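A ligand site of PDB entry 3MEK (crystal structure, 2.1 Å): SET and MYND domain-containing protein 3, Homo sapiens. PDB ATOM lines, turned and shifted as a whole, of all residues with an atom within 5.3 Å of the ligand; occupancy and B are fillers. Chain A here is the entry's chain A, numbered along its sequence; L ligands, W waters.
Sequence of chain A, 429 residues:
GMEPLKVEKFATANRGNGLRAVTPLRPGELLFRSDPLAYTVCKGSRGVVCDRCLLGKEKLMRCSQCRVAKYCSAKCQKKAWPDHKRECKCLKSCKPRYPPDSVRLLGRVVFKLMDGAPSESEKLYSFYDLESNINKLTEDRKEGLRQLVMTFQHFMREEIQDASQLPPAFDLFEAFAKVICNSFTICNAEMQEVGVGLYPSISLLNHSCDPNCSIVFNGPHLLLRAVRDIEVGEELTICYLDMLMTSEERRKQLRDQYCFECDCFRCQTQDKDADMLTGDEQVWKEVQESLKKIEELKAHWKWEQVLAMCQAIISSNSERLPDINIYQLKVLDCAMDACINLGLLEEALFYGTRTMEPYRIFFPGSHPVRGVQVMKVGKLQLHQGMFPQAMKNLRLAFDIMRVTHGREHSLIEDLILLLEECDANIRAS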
ATOM      1  N   ASN A  14     -21.736  -5.083  -1.313  1.00  0.00           N
ATOM      2  CA  ASN A  14     -20.895  -4.485  -2.360  1.00  0.00           C
ATOM      3  C   ASN A  14     -20.455  -5.367  -3.517  1.00  0.00           C
ATOM      4  O   ASN A  14     -19.493  -5.025  -4.221  1.00  0.00           O
ATOM      5  CB  ASN A  14     -19.681  -3.777  -1.759  1.00  0.00           C
ATOM      6  CG  ASN A  14     -18.824  -4.675  -0.883  1.00  0.00           C
ATOM      7  OD1 ASN A  14     -18.604  -5.865  -1.155  1.00  0.00           O
ATOM      8  ND2 ASN A  14     -18.313  -4.094   0.205  1.00  0.00           N
ATOM      9  N   ARG A  15     -21.095  -6.510  -3.711  1.00  0.00           N
ATOM     10  CA  ARG A  15     -20.755  -7.339  -4.851  1.00  0.00           C
ATOM     11  C   ARG A  15     -21.967  -7.963  -5.547  1.00  0.00           C
ATOM     12  O   ARG A  15     -21.909  -9.112  -5.962  1.00  0.00           O
ATOM     13  CB  ARG A  15     -19.671  -8.357  -4.508  1.00  0.00           C
ATOM     14  CG  ARG A  15     -19.816  -9.065  -3.202  1.00  0.00           C
ATOM     15  CD  ARG A  15     -18.437  -9.380  -2.672  1.00  0.00           C
ATOM     16  NE  ARG A  15     -18.441 -10.630  -1.921  1.00  0.00           N
ATOM     17  CZ  ARG A  15     -17.416 -11.088  -1.213  1.00  0.00           C
ATOM     18  NH1 ARG A  15     -16.282 -10.403  -1.135  1.00  0.00           N
ATOM     19  NH2 ARG A  15     -17.531 -12.242  -0.577  1.00  0.00           N
ATOM     20  N   GLY A  16     -23.028  -7.173  -5.681  1.00  0.00           N
ATOM     21  CA  GLY A  16     -24.244  -7.598  -6.352  1.00  0.00           C
ATOM     22  C   GLY A  16     -24.970  -8.714  -5.614  1.00  0.00           C
ATOM     23  O   GLY A  16     -25.061  -8.710  -4.364  1.00  0.00           O
ATOM     24  N   ASN A  17     -25.514  -9.657  -6.369  1.00  0.00           N
ATOM     25  CA  ASN A  17     -26.192 -10.784  -5.765  1.00  0.00           C
ATOM     26  C   ASN A  17     -25.205 -11.862  -5.400  1.00  0.00           C
ATOM     27  O   ASN A  17     -24.117 -11.949  -5.980  1.00  0.00           O
ATOM     28  CB  ASN A  17     -27.322 -11.320  -6.684  1.00  0.00           C
ATOM     29  CG  ASN A  17     -28.355 -10.264  -7.014  1.00  0.00           C
ATOM     30  OD1 ASN A  17     -28.695 -10.064  -8.176  1.00  0.00           O
ATOM     31  ND2 ASN A  17     -28.821  -9.564  -5.994  1.00  0.00           N
ATOM     32  N   GLY A  18     -25.567 -12.679  -4.414  1.00  0.00           N
ATOM     33  CA  GLY A  18     -24.727 -13.807  -4.007  1.00  0.00           C
ATOM     34  C   GLY A  18     -25.598 -14.958  -3.529  1.00  0.00           C
ATOM     35  O   GLY A  18     -26.809 -14.899  -3.605  1.00  0.00           O
ATOM     36  N   TYR A 125     -31.757 -18.187 -10.612  1.00  0.00           N
ATOM     37  CA  TYR A 125     -31.234 -17.010 -11.308  1.00  0.00           C
ATOM     38  C   TYR A 125     -31.236 -17.404 -12.786  1.00  0.00           C
ATOM     39  O   TYR A 125     -30.801 -18.513 -13.134  1.00  0.00           O
ATOM     40  CB  TYR A 125     -29.775 -16.802 -10.857  1.00  0.00           C
ATOM     41  CG  TYR A 125     -29.231 -15.379 -10.796  1.00  0.00           C
ATOM     42  CD1 TYR A 125     -29.950 -14.340 -10.210  1.00  0.00           C
ATOM     43  CD2 TYR A 125     -27.917 -15.109 -11.252  1.00  0.00           C
ATOM     44  CE1 TYR A 125     -29.416 -13.059 -10.117  1.00  0.00           C
ATOM     45  CE2 TYR A 125     -27.376 -13.842 -11.177  1.00  0.00           C
ATOM     46  CZ  TYR A 125     -28.129 -12.810 -10.600  1.00  0.00           C
ATOM     47  OH  TYR A 125     -27.588 -11.547 -10.500  1.00  0.00           O
ATOM     48  N   ASP A 129     -31.051 -12.416 -15.638  1.00  0.00           N
ATOM     49  CA  ASP A 129     -30.571 -11.809 -14.394  1.00  0.00           C
ATOM     50  C   ASP A 129     -29.052 -11.646 -14.337  1.00  0.00           C
ATOM     51  O   ASP A 129     -28.544 -10.906 -13.491  1.00  0.00           O
ATOM     52  CB  ASP A 129     -31.000 -12.667 -13.200  1.00  0.00           C
ATOM     53  CG  ASP A 129     -32.512 -12.806 -13.088  1.00  0.00           C
ATOM     54  OD1 ASP A 129     -33.220 -11.805 -13.328  1.00  0.00           O
ATOM     55  OD2 ASP A 129     -32.982 -13.919 -12.754  1.00  0.00           O
ATOM     56  N   LEU A 130     -28.327 -12.352 -15.202  1.00  0.00           N
ATOM     57  CA  LEU A 130     -26.860 -12.456 -15.088  1.00  0.00           C
ATOM     58  C   LEU A 130     -26.192 -11.088 -15.118  1.00  0.00           C
ATOM     59  O   LEU A 130     -26.643 -10.201 -15.845  1.00  0.00           O
ATOM     60  CB  LEU A 130     -26.271 -13.329 -16.178  1.00  0.00           C
ATOM     61  CG  LEU A 130     -26.556 -14.827 -16.188  1.00  0.00           C
ATOM     62  CD1 LEU A 130     -25.844 -15.458 -17.400  1.00  0.00           C
ATOM     63  CD2 LEU A 130     -26.118 -15.496 -14.886  1.00  0.00           C
ATOM     64  N   GLU A 131     -25.132 -10.925 -14.339  1.00  0.00           N
ATOM     65  CA  GLU A 131     -24.349  -9.685 -14.321  1.00  0.00           C
ATOM     66  C   GLU A 131     -23.635  -9.509 -15.651  1.00  0.00           C
ATOM     67  O   GLU A 131     -23.060 -10.459 -16.191  1.00  0.00           O
ATOM     68  CB  GLU A 131     -23.332  -9.715 -13.169  1.00  0.00           C
ATOM     69  CG  GLU A 131     -22.371  -8.521 -13.114  1.00  0.00           C
ATOM     70  CD  GLU A 131     -23.099  -7.239 -12.749  1.00  0.00           C
ATOM     71  OE1 GLU A 131     -23.491  -7.116 -11.568  1.00  0.00           O
ATOM     72  OE2 GLU A 131     -23.279  -6.353 -13.633  1.00  0.00           O
ATOM     73  N   ASN A 133     -21.712  -6.341 -16.121  1.00  0.00           N
ATOM     74  CA  ASN A 133     -20.700  -5.319 -15.855  1.00  0.00           C
ATOM     75  C   ASN A 133     -20.582  -4.210 -16.914  1.00  0.00           C
ATOM     76  O   ASN A 133     -19.498  -3.658 -17.102  1.00  0.00           O
ATOM     77  CB  ASN A 133     -19.320  -5.948 -15.625  1.00  0.00           C
ATOM     78  CG  ASN A 133     -19.265  -6.833 -14.399  1.00  0.00           C
ATOM     79  OD1 ASN A 133     -18.792  -7.969 -14.462  1.00  0.00           O
ATOM     80  ND2 ASN A 133     -19.753  -6.326 -13.274  1.00  0.00           N
ATOM     81  N   CYS A 181     -18.270 -12.845 -18.313  1.00  0.00           N
ATOM     82  CA  CYS A 181     -18.057 -12.968 -16.887  1.00  0.00           C
ATOM     83  C   CYS A 181     -18.849 -14.110 -16.243  1.00  0.00           C
ATOM     84  O   CYS A 181     -18.809 -14.290 -15.003  1.00  0.00           O
ATOM     85  CB  CYS A 181     -18.323 -11.643 -16.175  1.00  0.00           C
ATOM     86  SG  CYS A 181     -20.009 -11.030 -16.287  1.00  0.00           S
ATOM     87  N   ASN A 182     -19.553 -14.889 -17.049  1.00  0.00           N
ATOM     88  CA  ASN A 182     -20.356 -15.977 -16.472  1.00  0.00           C
ATOM     89  C   ASN A 182     -20.076 -17.359 -17.060  1.00  0.00           C
ATOM     90  O   ASN A 182     -20.674 -18.322 -16.655  1.00  0.00           O
ATOM     91  CB  ASN A 182     -21.861 -15.634 -16.535  1.00  0.00           C
ATOM     92  CG  ASN A 182     -22.226 -14.495 -15.631  1.00  0.00           C
ATOM     93  OD1 ASN A 182     -22.303 -14.667 -14.418  1.00  0.00           O
ATOM     94  ND2 ASN A 182     -22.452 -13.308 -16.196  1.00  0.00           N
ATOM     95  N   SER A 203     -24.026 -19.156 -11.146  1.00  0.00           N
ATOM     96  CA  SER A 203     -23.449 -17.824 -11.337  1.00  0.00           C
ATOM     97  C   SER A 203     -23.689 -16.874 -10.167  1.00  0.00           C
ATOM     98  O   SER A 203     -23.093 -15.798 -10.123  1.00  0.00           O
ATOM     99  CB  SER A 203     -23.979 -17.185 -12.611  1.00  0.00           C
ATOM    100  OG  SER A 203     -23.242 -17.668 -13.716  1.00  0.00           O
ATOM    101  N   LEU A 204     -24.569 -17.254  -9.242  1.00  0.00           N
ATOM    102  CA  LEU A 204     -24.741 -16.482  -8.011  1.00  0.00           C
ATOM    103  C   LEU A 204     -23.534 -16.510  -7.073  1.00  0.00           C
ATOM    104  O   LEU A 204     -23.390 -15.641  -6.249  1.00  0.00           O
ATOM    105  CB  LEU A 204     -26.011 -16.932  -7.259  1.00  0.00           C
ATOM    106  CG  LEU A 204     -27.318 -16.339  -7.766  1.00  0.00           C
ATOM    107  CD1 LEU A 204     -28.555 -17.028  -7.131  1.00  0.00           C
ATOM    108  CD2 LEU A 204     -27.374 -14.819  -7.509  1.00  0.00           C
ATOM    109  N   LEU A 205     -22.696 -17.533  -7.179  1.00  0.00           N
ATOM    110  CA  LEU A 205     -21.493 -17.605  -6.334  1.00  0.00           C
ATOM    111  C   LEU A 205     -20.482 -16.509  -6.680  1.00  0.00           C
ATOM    112  O   LEU A 205     -19.972 -16.446  -7.798  1.00  0.00           O
ATOM    113  CB  LEU A 205     -20.838 -18.984  -6.407  1.00  0.00           C
ATOM    114  CG  LEU A 205     -21.710 -20.155  -5.920  1.00  0.00           C
ATOM    115  CD1 LEU A 205     -21.351 -21.369  -6.732  1.00  0.00           C
ATOM    116  CD2 LEU A 205     -21.538 -20.419  -4.453  1.00  0.00           C
ATOM    117  N   ASN A 206     -20.210 -15.659  -5.702  1.00  0.00           N
ATOM    118  CA  ASN A 206     -19.122 -14.703  -5.779  1.00  0.00           C
ATOM    119  C   ASN A 206     -17.745 -15.360  -5.525  1.00  0.00           C
ATOM    120  O   ASN A 206     -17.664 -16.490  -5.046  1.00  0.00           O
ATOM    121  CB  ASN A 206     -19.382 -13.533  -4.817  1.00  0.00           C
ATOM    122  CG  ASN A 206     -20.471 -12.597  -5.338  1.00  0.00           C
ATOM    123  OD1 ASN A 206     -20.465 -12.202  -6.506  1.00  0.00           O
ATOM    124  ND2 ASN A 206     -21.445 -12.279  -4.486  1.00  0.00           N
ATOM    125  N   HIS A 207     -16.690 -14.646  -5.880  1.00  0.00           N
ATOM    126  CA  HIS A 207     -15.335 -15.212  -5.877  1.00  0.00           C
ATOM    127  C   HIS A 207     -14.642 -14.994  -4.540  1.00  0.00           C
ATOM    128  O   HIS A 207     -14.854 -13.989  -3.902  1.00  0.00           O
ATOM    129  CB  HIS A 207     -14.480 -14.531  -6.965  1.00  0.00           C
ATOM    130  CG  HIS A 207     -13.001 -14.688  -6.752  1.00  0.00           C
ATOM    131  ND1 HIS A 207     -12.306 -15.778  -7.217  1.00  0.00           N
ATOM    132  CD2 HIS A 207     -12.101 -13.905  -6.094  1.00  0.00           C
ATOM    133  CE1 HIS A 207     -11.029 -15.653  -6.881  1.00  0.00           C
ATOM    134  NE2 HIS A 207     -10.875 -14.529  -6.198  1.00  0.00           N
ATOM    135  N   SER A 208     -13.795 -15.942  -4.149  1.00  0.00           N
ATOM    136  CA  SER A 208     -12.832 -15.760  -3.078  1.00  0.00           C
ATOM    137  C   SER A 208     -11.547 -16.523  -3.407  1.00  0.00           C
ATOM    138  O   SER A 208     -11.601 -17.648  -3.880  1.00  0.00           O
ATOM    139  CB  SER A 208     -13.377 -16.288  -1.762  1.00  0.00           C
ATOM    140  OG  SER A 208     -12.382 -16.175  -0.771  1.00  0.00           O
ATOM    141  N   TYR A 240     -12.776 -18.467  -8.665  1.00  0.00           N
ATOM    142  CA  TYR A 240     -12.970 -18.413 -10.121  1.00  0.00           C
ATOM    143  C   TYR A 240     -11.727 -18.852 -10.903  1.00  0.00           C
ATOM    144  O   TYR A 240     -11.824 -19.111 -12.086  1.00  0.00           O
ATOM    145  CB  TYR A 240     -13.307 -16.970 -10.555  1.00  0.00           C
ATOM    146  CG  TYR A 240     -14.680 -16.435 -10.142  1.00  0.00           C
ATOM    147  CD1 TYR A 240     -15.584 -17.188  -9.381  1.00  0.00           C
ATOM    148  CD2 TYR A 240     -15.055 -15.132 -10.501  1.00  0.00           C
ATOM    149  CE1 TYR A 240     -16.826 -16.654  -9.005  1.00  0.00           C
ATOM    150  CE2 TYR A 240     -16.280 -14.609 -10.147  1.00  0.00           C
ATOM    151  CZ  TYR A 240     -17.157 -15.367  -9.403  1.00  0.00           C
ATOM    152  OH  TYR A 240     -18.363 -14.786  -9.071  1.00  0.00           O
ATOM    153  N   GLN A 257     -11.572  -9.963 -16.847  1.00  0.00           N
ATOM    154  CA  GLN A 257     -12.706 -10.808 -17.170  1.00  0.00           C
ATOM    155  C   GLN A 257     -13.950 -10.495 -16.319  1.00  0.00           C
ATOM    156  O   GLN A 257     -15.102 -10.618 -16.784  1.00  0.00           O
ATOM    157  CB  GLN A 257     -12.297 -12.267 -17.057  1.00  0.00           C
ATOM    158  CG  GLN A 257     -13.468 -13.227 -17.124  1.00  0.00           C
ATOM    159  CD  GLN A 257     -13.053 -14.680 -17.310  1.00  0.00           C
ATOM    160  OE1 GLN A 257     -11.880 -15.043 -17.142  1.00  0.00           O
ATOM    161  NE2 GLN A 257     -14.008 -15.527 -17.639  1.00  0.00           N
ATOM    162  N   TYR A 258     -13.710 -10.095 -15.071  1.00  0.00           N
ATOM    163  CA  TYR A 258     -14.810  -9.990 -14.110  1.00  0.00           C
ATOM    164  C   TYR A 258     -15.030  -8.594 -13.557  1.00  0.00           C
ATOM    165  O   TYR A 258     -15.966  -8.383 -12.770  1.00  0.00           O
ATOM    166  CB  TYR A 258     -14.582 -10.962 -12.962  1.00  0.00           C
ATOM    167  CG  TYR A 258     -14.578 -12.437 -13.360  1.00  0.00           C
ATOM    168  CD1 TYR A 258     -15.766 -13.107 -13.634  1.00  0.00           C
ATOM    169  CD2 TYR A 258     -13.374 -13.143 -13.443  1.00  0.00           C
ATOM    170  CE1 TYR A 258     -15.773 -14.450 -13.965  1.00  0.00           C
ATOM    171  CE2 TYR A 258     -13.350 -14.487 -13.782  1.00  0.00           C
ATOM    172  CZ  TYR A 258     -14.561 -15.141 -14.045  1.00  0.00           C
ATOM    173  OH  TYR A 258     -14.569 -16.471 -14.369  1.00  0.00           O
ATOM    174  N   CYS A 259     -14.200  -7.650 -13.986  1.00  0.00           N
ATOM    175  CA  CYS A 259     -14.343  -6.237 -13.587  1.00  0.00           C
ATOM    176  C   CYS A 259     -14.443  -5.993 -12.080  1.00  0.00           C
ATOM    177  O   CYS A 259     -15.303  -5.216 -11.618  1.00  0.00           O
ATOM    178  CB  CYS A 259     -15.519  -5.567 -14.314  1.00  0.00           C
ATOM    179  SG  CYS A 259     -15.391  -5.577 -16.118  1.00  0.00           S
ATOM    180  N   PHE A 260     -13.603  -6.648 -11.309  1.00  0.00           N
ATOM    181  CA  PHE A 260     -13.491  -6.260  -9.894  1.00  0.00           C
ATOM    182  C   PHE A 260     -12.087  -6.396  -9.339  1.00  0.00           C
ATOM    183  O   PHE A 260     -11.226  -7.032  -9.967  1.00  0.00           O
ATOM    184  CB  PHE A 260     -14.530  -6.985  -9.005  1.00  0.00           C
ATOM    185  CG  PHE A 260     -14.189  -8.413  -8.738  1.00  0.00           C
ATOM    186  CD1 PHE A 260     -13.431  -8.765  -7.626  1.00  0.00           C
ATOM    187  CD2 PHE A 260     -14.616  -9.423  -9.610  1.00  0.00           C
ATOM    188  CE1 PHE A 260     -13.103 -10.068  -7.379  1.00  0.00           C
ATOM    189  CE2 PHE A 260     -14.287 -10.759  -9.359  1.00  0.00           C
ATOM    190  CZ  PHE A 260     -13.521 -11.078  -8.230  1.00  0.00           C
ATOM    191  N   GLU A 261     -11.880  -5.774  -8.171  1.00  0.00           N
ATOM    192  CA  GLU A 261     -10.628  -5.778  -7.428  1.00  0.00           C
ATOM    193  C   GLU A 261     -10.885  -6.641  -6.201  1.00  0.00           C
ATOM    194  O   GLU A 261     -11.851  -6.419  -5.479  1.00  0.00           O
ATOM    195  CB  GLU A 261     -10.238  -4.341  -6.978  1.00  0.00           C
ATOM    196  CG  GLU A 261     -10.566  -3.201  -8.003  1.00  0.00           C
ATOM    197  CD  GLU A 261      -9.735  -3.298  -9.276  1.00  0.00           C
ATOM    198  OE1 GLU A 261      -8.690  -4.010  -9.231  1.00  0.00           O
ATOM    199  OE2 GLU A 261     -10.120  -2.687 -10.306  1.00  0.00           O
ATOM    200  N   CYS A 262     -10.030  -7.628  -5.976  1.00  0.00           N
ATOM    201  CA  CYS A 262     -10.237  -8.522  -4.841  1.00  0.00           C
ATOM    202  C   CYS A 262      -9.594  -7.939  -3.576  1.00  0.00           C
ATOM    203  O   CYS A 262      -8.421  -7.605  -3.577  1.00  0.00           O
ATOM    204  CB  CYS A 262      -9.677  -9.917  -5.151  1.00  0.00           C
ATOM    205  SG  CYS A 262     -10.148 -11.106  -3.863  1.00  0.00           S
HETATM  206  N1  LIG L   1     -22.449 -10.871  -7.925  1.00  0.00           N
HETATM  207  C1  LIG L   1     -22.871 -11.550  -9.188  1.00  0.00           C
HETATM  208  C2  LIG L   1     -24.267 -11.106  -9.612  1.00  0.00           C
HETATM  209  O1  LIG L   1     -24.800 -10.157  -9.027  1.00  0.00           O
HETATM  210  O2  LIG L   1     -24.873 -11.640 -10.569  1.00  0.00           O
HETATM  211  C3  LIG L   1     -22.750 -13.050  -8.984  1.00  0.00           C
HETATM  212  C4  LIG L   1     -21.365 -13.558  -9.401  1.00  0.00           C
HETATM  213  S1  LIG L   1     -21.075 -13.427 -11.202  1.00  0.00           S
HETATM  214  C5  LIG L   1     -20.496 -15.096 -11.609  1.00  0.00           C
HETATM  215  C6  LIG L   1     -19.461 -12.571 -11.282  1.00  0.00           C
HETATM  216  C7  LIG L   1     -19.485 -11.082 -10.918  1.00  0.00           C
HETATM  217  O3  LIG L   1     -19.784 -10.857  -9.550  1.00  0.00           O
HETATM  218  C8  LIG L   1     -18.152 -10.350 -11.135  1.00  0.00           C
HETATM  219  O4  LIG L   1     -18.050  -9.925 -12.481  1.00  0.00           O
HETATM  220  C9  LIG L   1     -18.272  -9.184 -10.165  1.00  0.00           C
HETATM  221  O5  LIG L   1     -19.147  -8.227 -10.700  1.00  0.00           O
HETATM  222  C10 LIG L   1     -19.004  -9.819  -8.996  1.00  0.00           C
HETATM  223  N2  LIG L   1     -18.088 -10.413  -8.002  1.00  0.00           N
HETATM  224  C11 LIG L   1     -17.804 -11.745  -7.854  1.00  0.00           C
HETATM  225  N3  LIG L   1     -16.948 -11.879  -6.835  1.00  0.00           N
HETATM  226  C12 LIG L   1     -16.662 -10.665  -6.334  1.00  0.00           C
HETATM  227  C13 LIG L   1     -15.838 -10.261  -5.301  1.00  0.00           C
HETATM  228  N4  LIG L   1     -15.128 -11.132  -4.565  1.00  0.00           N
HETATM  229  N5  LIG L   1     -15.753  -8.907  -5.044  1.00  0.00           N
HETATM  230  C14 LIG L   1     -16.478  -7.983  -5.777  1.00  0.00           C
HETATM  231  N6  LIG L   1     -17.300  -8.404  -6.791  1.00  0.00           N
HETATM  232  C15 LIG L   1     -17.379  -9.726  -7.065  1.00  0.00           C
HETATM  233  O   HOH W   1     -18.049  -6.131  -8.006  1.00  0.00           O
HETATM  234  O   HOH W   2     -26.025  -8.254 -10.243  1.00  0.00           O
HETATM  235  O   HOH W   3     -12.890 -10.582  -2.620  1.00  0.00           O
HETATM  236  O   HOH W   4     -16.429  -5.223  -3.650  1.00  0.00           O
HETATM  237  O   HOH W   5     -24.248 -13.044 -12.802  1.00  0.00           O
HETATM  238  O   HOH W   6     -13.701  -7.518  -3.631  1.00  0.00           O
HETATM  239  O   HOH W   7     -22.045  -8.272  -9.483  1.00  0.00           O
HETATM  240  O   HOH W   8     -17.870  -5.811 -10.995  1.00  0.00           O
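O4 of the ligand lies within hydrogen-bond range of O of Tyr 258, at 2.6 Å.
The backbone carbonyl oxygen (O) of Arg 15 sits at hydrogen-bond distance from a nitrogen (N1) of the ligand (2.7 Å).
The side-chain hydroxyl of Tyr 125 is in hydrogen-bond range of an oxygen (O2) of the ligand, at 2.7 Å.
N1 of the ligand lies within hydrogen-bond range of OD1 of Asn 206 (2.8 Å).
N of Asn 17 is in hydrogen-bond range of O1 of the ligand, at 2.8 Å.
N1 of the ligand sits at hydrogen-bond distance from O of Asn 17 (2.8 Å).
The side-chain amide oxygen of Asn 133 lies within hydrogen-bond range of an oxygen (O4) of the ligand.
N3 of the ligand sits at hydrogen-bond distance from N of His 207 (2.9 Å).
The backbone carbonyl oxygen of His 207 lies within hydrogen-bond range of a nitrogen (N4) of the ligand.
OH of Tyr 258 sits at hydrogen-bond distance from NE2 of Gln 257 (3.4 Å).
The backbone carbonyl oxygen (O) of Arg 15 sits close to the side-chain amide oxygen (OD1) of Asn 206, at 3.5 Å.
OH of Tyr 125 lies within hydrogen-bond range of OD1 of Asn 17 (3.0 Å).
The side-chain amide nitrogen (ND2) of Asn 206 lies within hydrogen-bond range of the backbone carbonyl oxygen (O) of Asn 17.
The backbone NH of Asn 133 lies within hydrogen-bond range of the side-chain carboxylate of Glu 131, 2.9 Å away.
OG of Ser 203 lies within hydrogen-bond range of OD1 of Asn 182, 3.2 Å away.
The side-chain amide nitrogen (ND2) of Asn 182 lies within hydrogen-bond range of the backbone carbonyl oxygen (O) of Glu 131, at 2.9 Å.
The side-chain amide nitrogen (ND2) of Asn 182 lies within hydrogen-bond range of the side-chain sulfur (SG) of Cys 181.
The side-chain amide oxygen (OD1) of Asn 182 sits close to a sulfur (S1) of the ligand (3.7 Å).
The backbone carbonyl oxygen of Ser 203 lies close to a sulfur (S1) of the ligand (3.3 Å).
The side-chain hydroxyl (OH) of Tyr 240 sits close to a sulfur (S1) of the ligand, 3.7 Å away.
Residues that only touch the ligand: Gly 16, Glu 131, Cys 181, Leu 204, Leu 205 and Phe 260.
Hydrophobic or aromatic side chains that line the ligand: Tyr 125, His 207, Tyr 240, Tyr 258 and Phe 260.
16 residues have an atom within 4 Å of the ligand: Arg 15, Gly 16, Asn 17, Tyr 125, Glu 131, Asn 133, Cys 181, Asn 182, Ser 203, Leu 204, Leu 205, Asn 206, His 207, Tyr 240, Tyr 258 and Phe 260.
Along chain A the residues within 4 Å of the ligand span positions 15 to 260.
Water W2 lies within hydrogen-bond range of O1 of the ligand (2.6 Å) and OE1 of Glu 131 (3.1 Å).
Water W5 lies within hydrogen-bond range of an oxygen (O2) of the ligand, the backbone NH (N) of Glu 131 and the side-chain amide oxygen (OD1) of Asn 182.
Water W8 lies within hydrogen-bond range of the backbone carbonyl oxygen (O) of Cys 259 (2.7 Å), an oxygen (O5) of the ligand (2.7 Å) and the side-chain amide nitrogen (ND2) of Asn 133 (3.0 Å).
Water W6 lies within hydrogen-bond range of O of Glu 261 (2.8 Å) and N5 of the ligand (2.9 Å).
Water W7 lies within hydrogen-bond range of the side-chain carboxylate of Glu 131 (2.8 Å) and a nitrogen (N1) of the ligand (3.1 Å).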
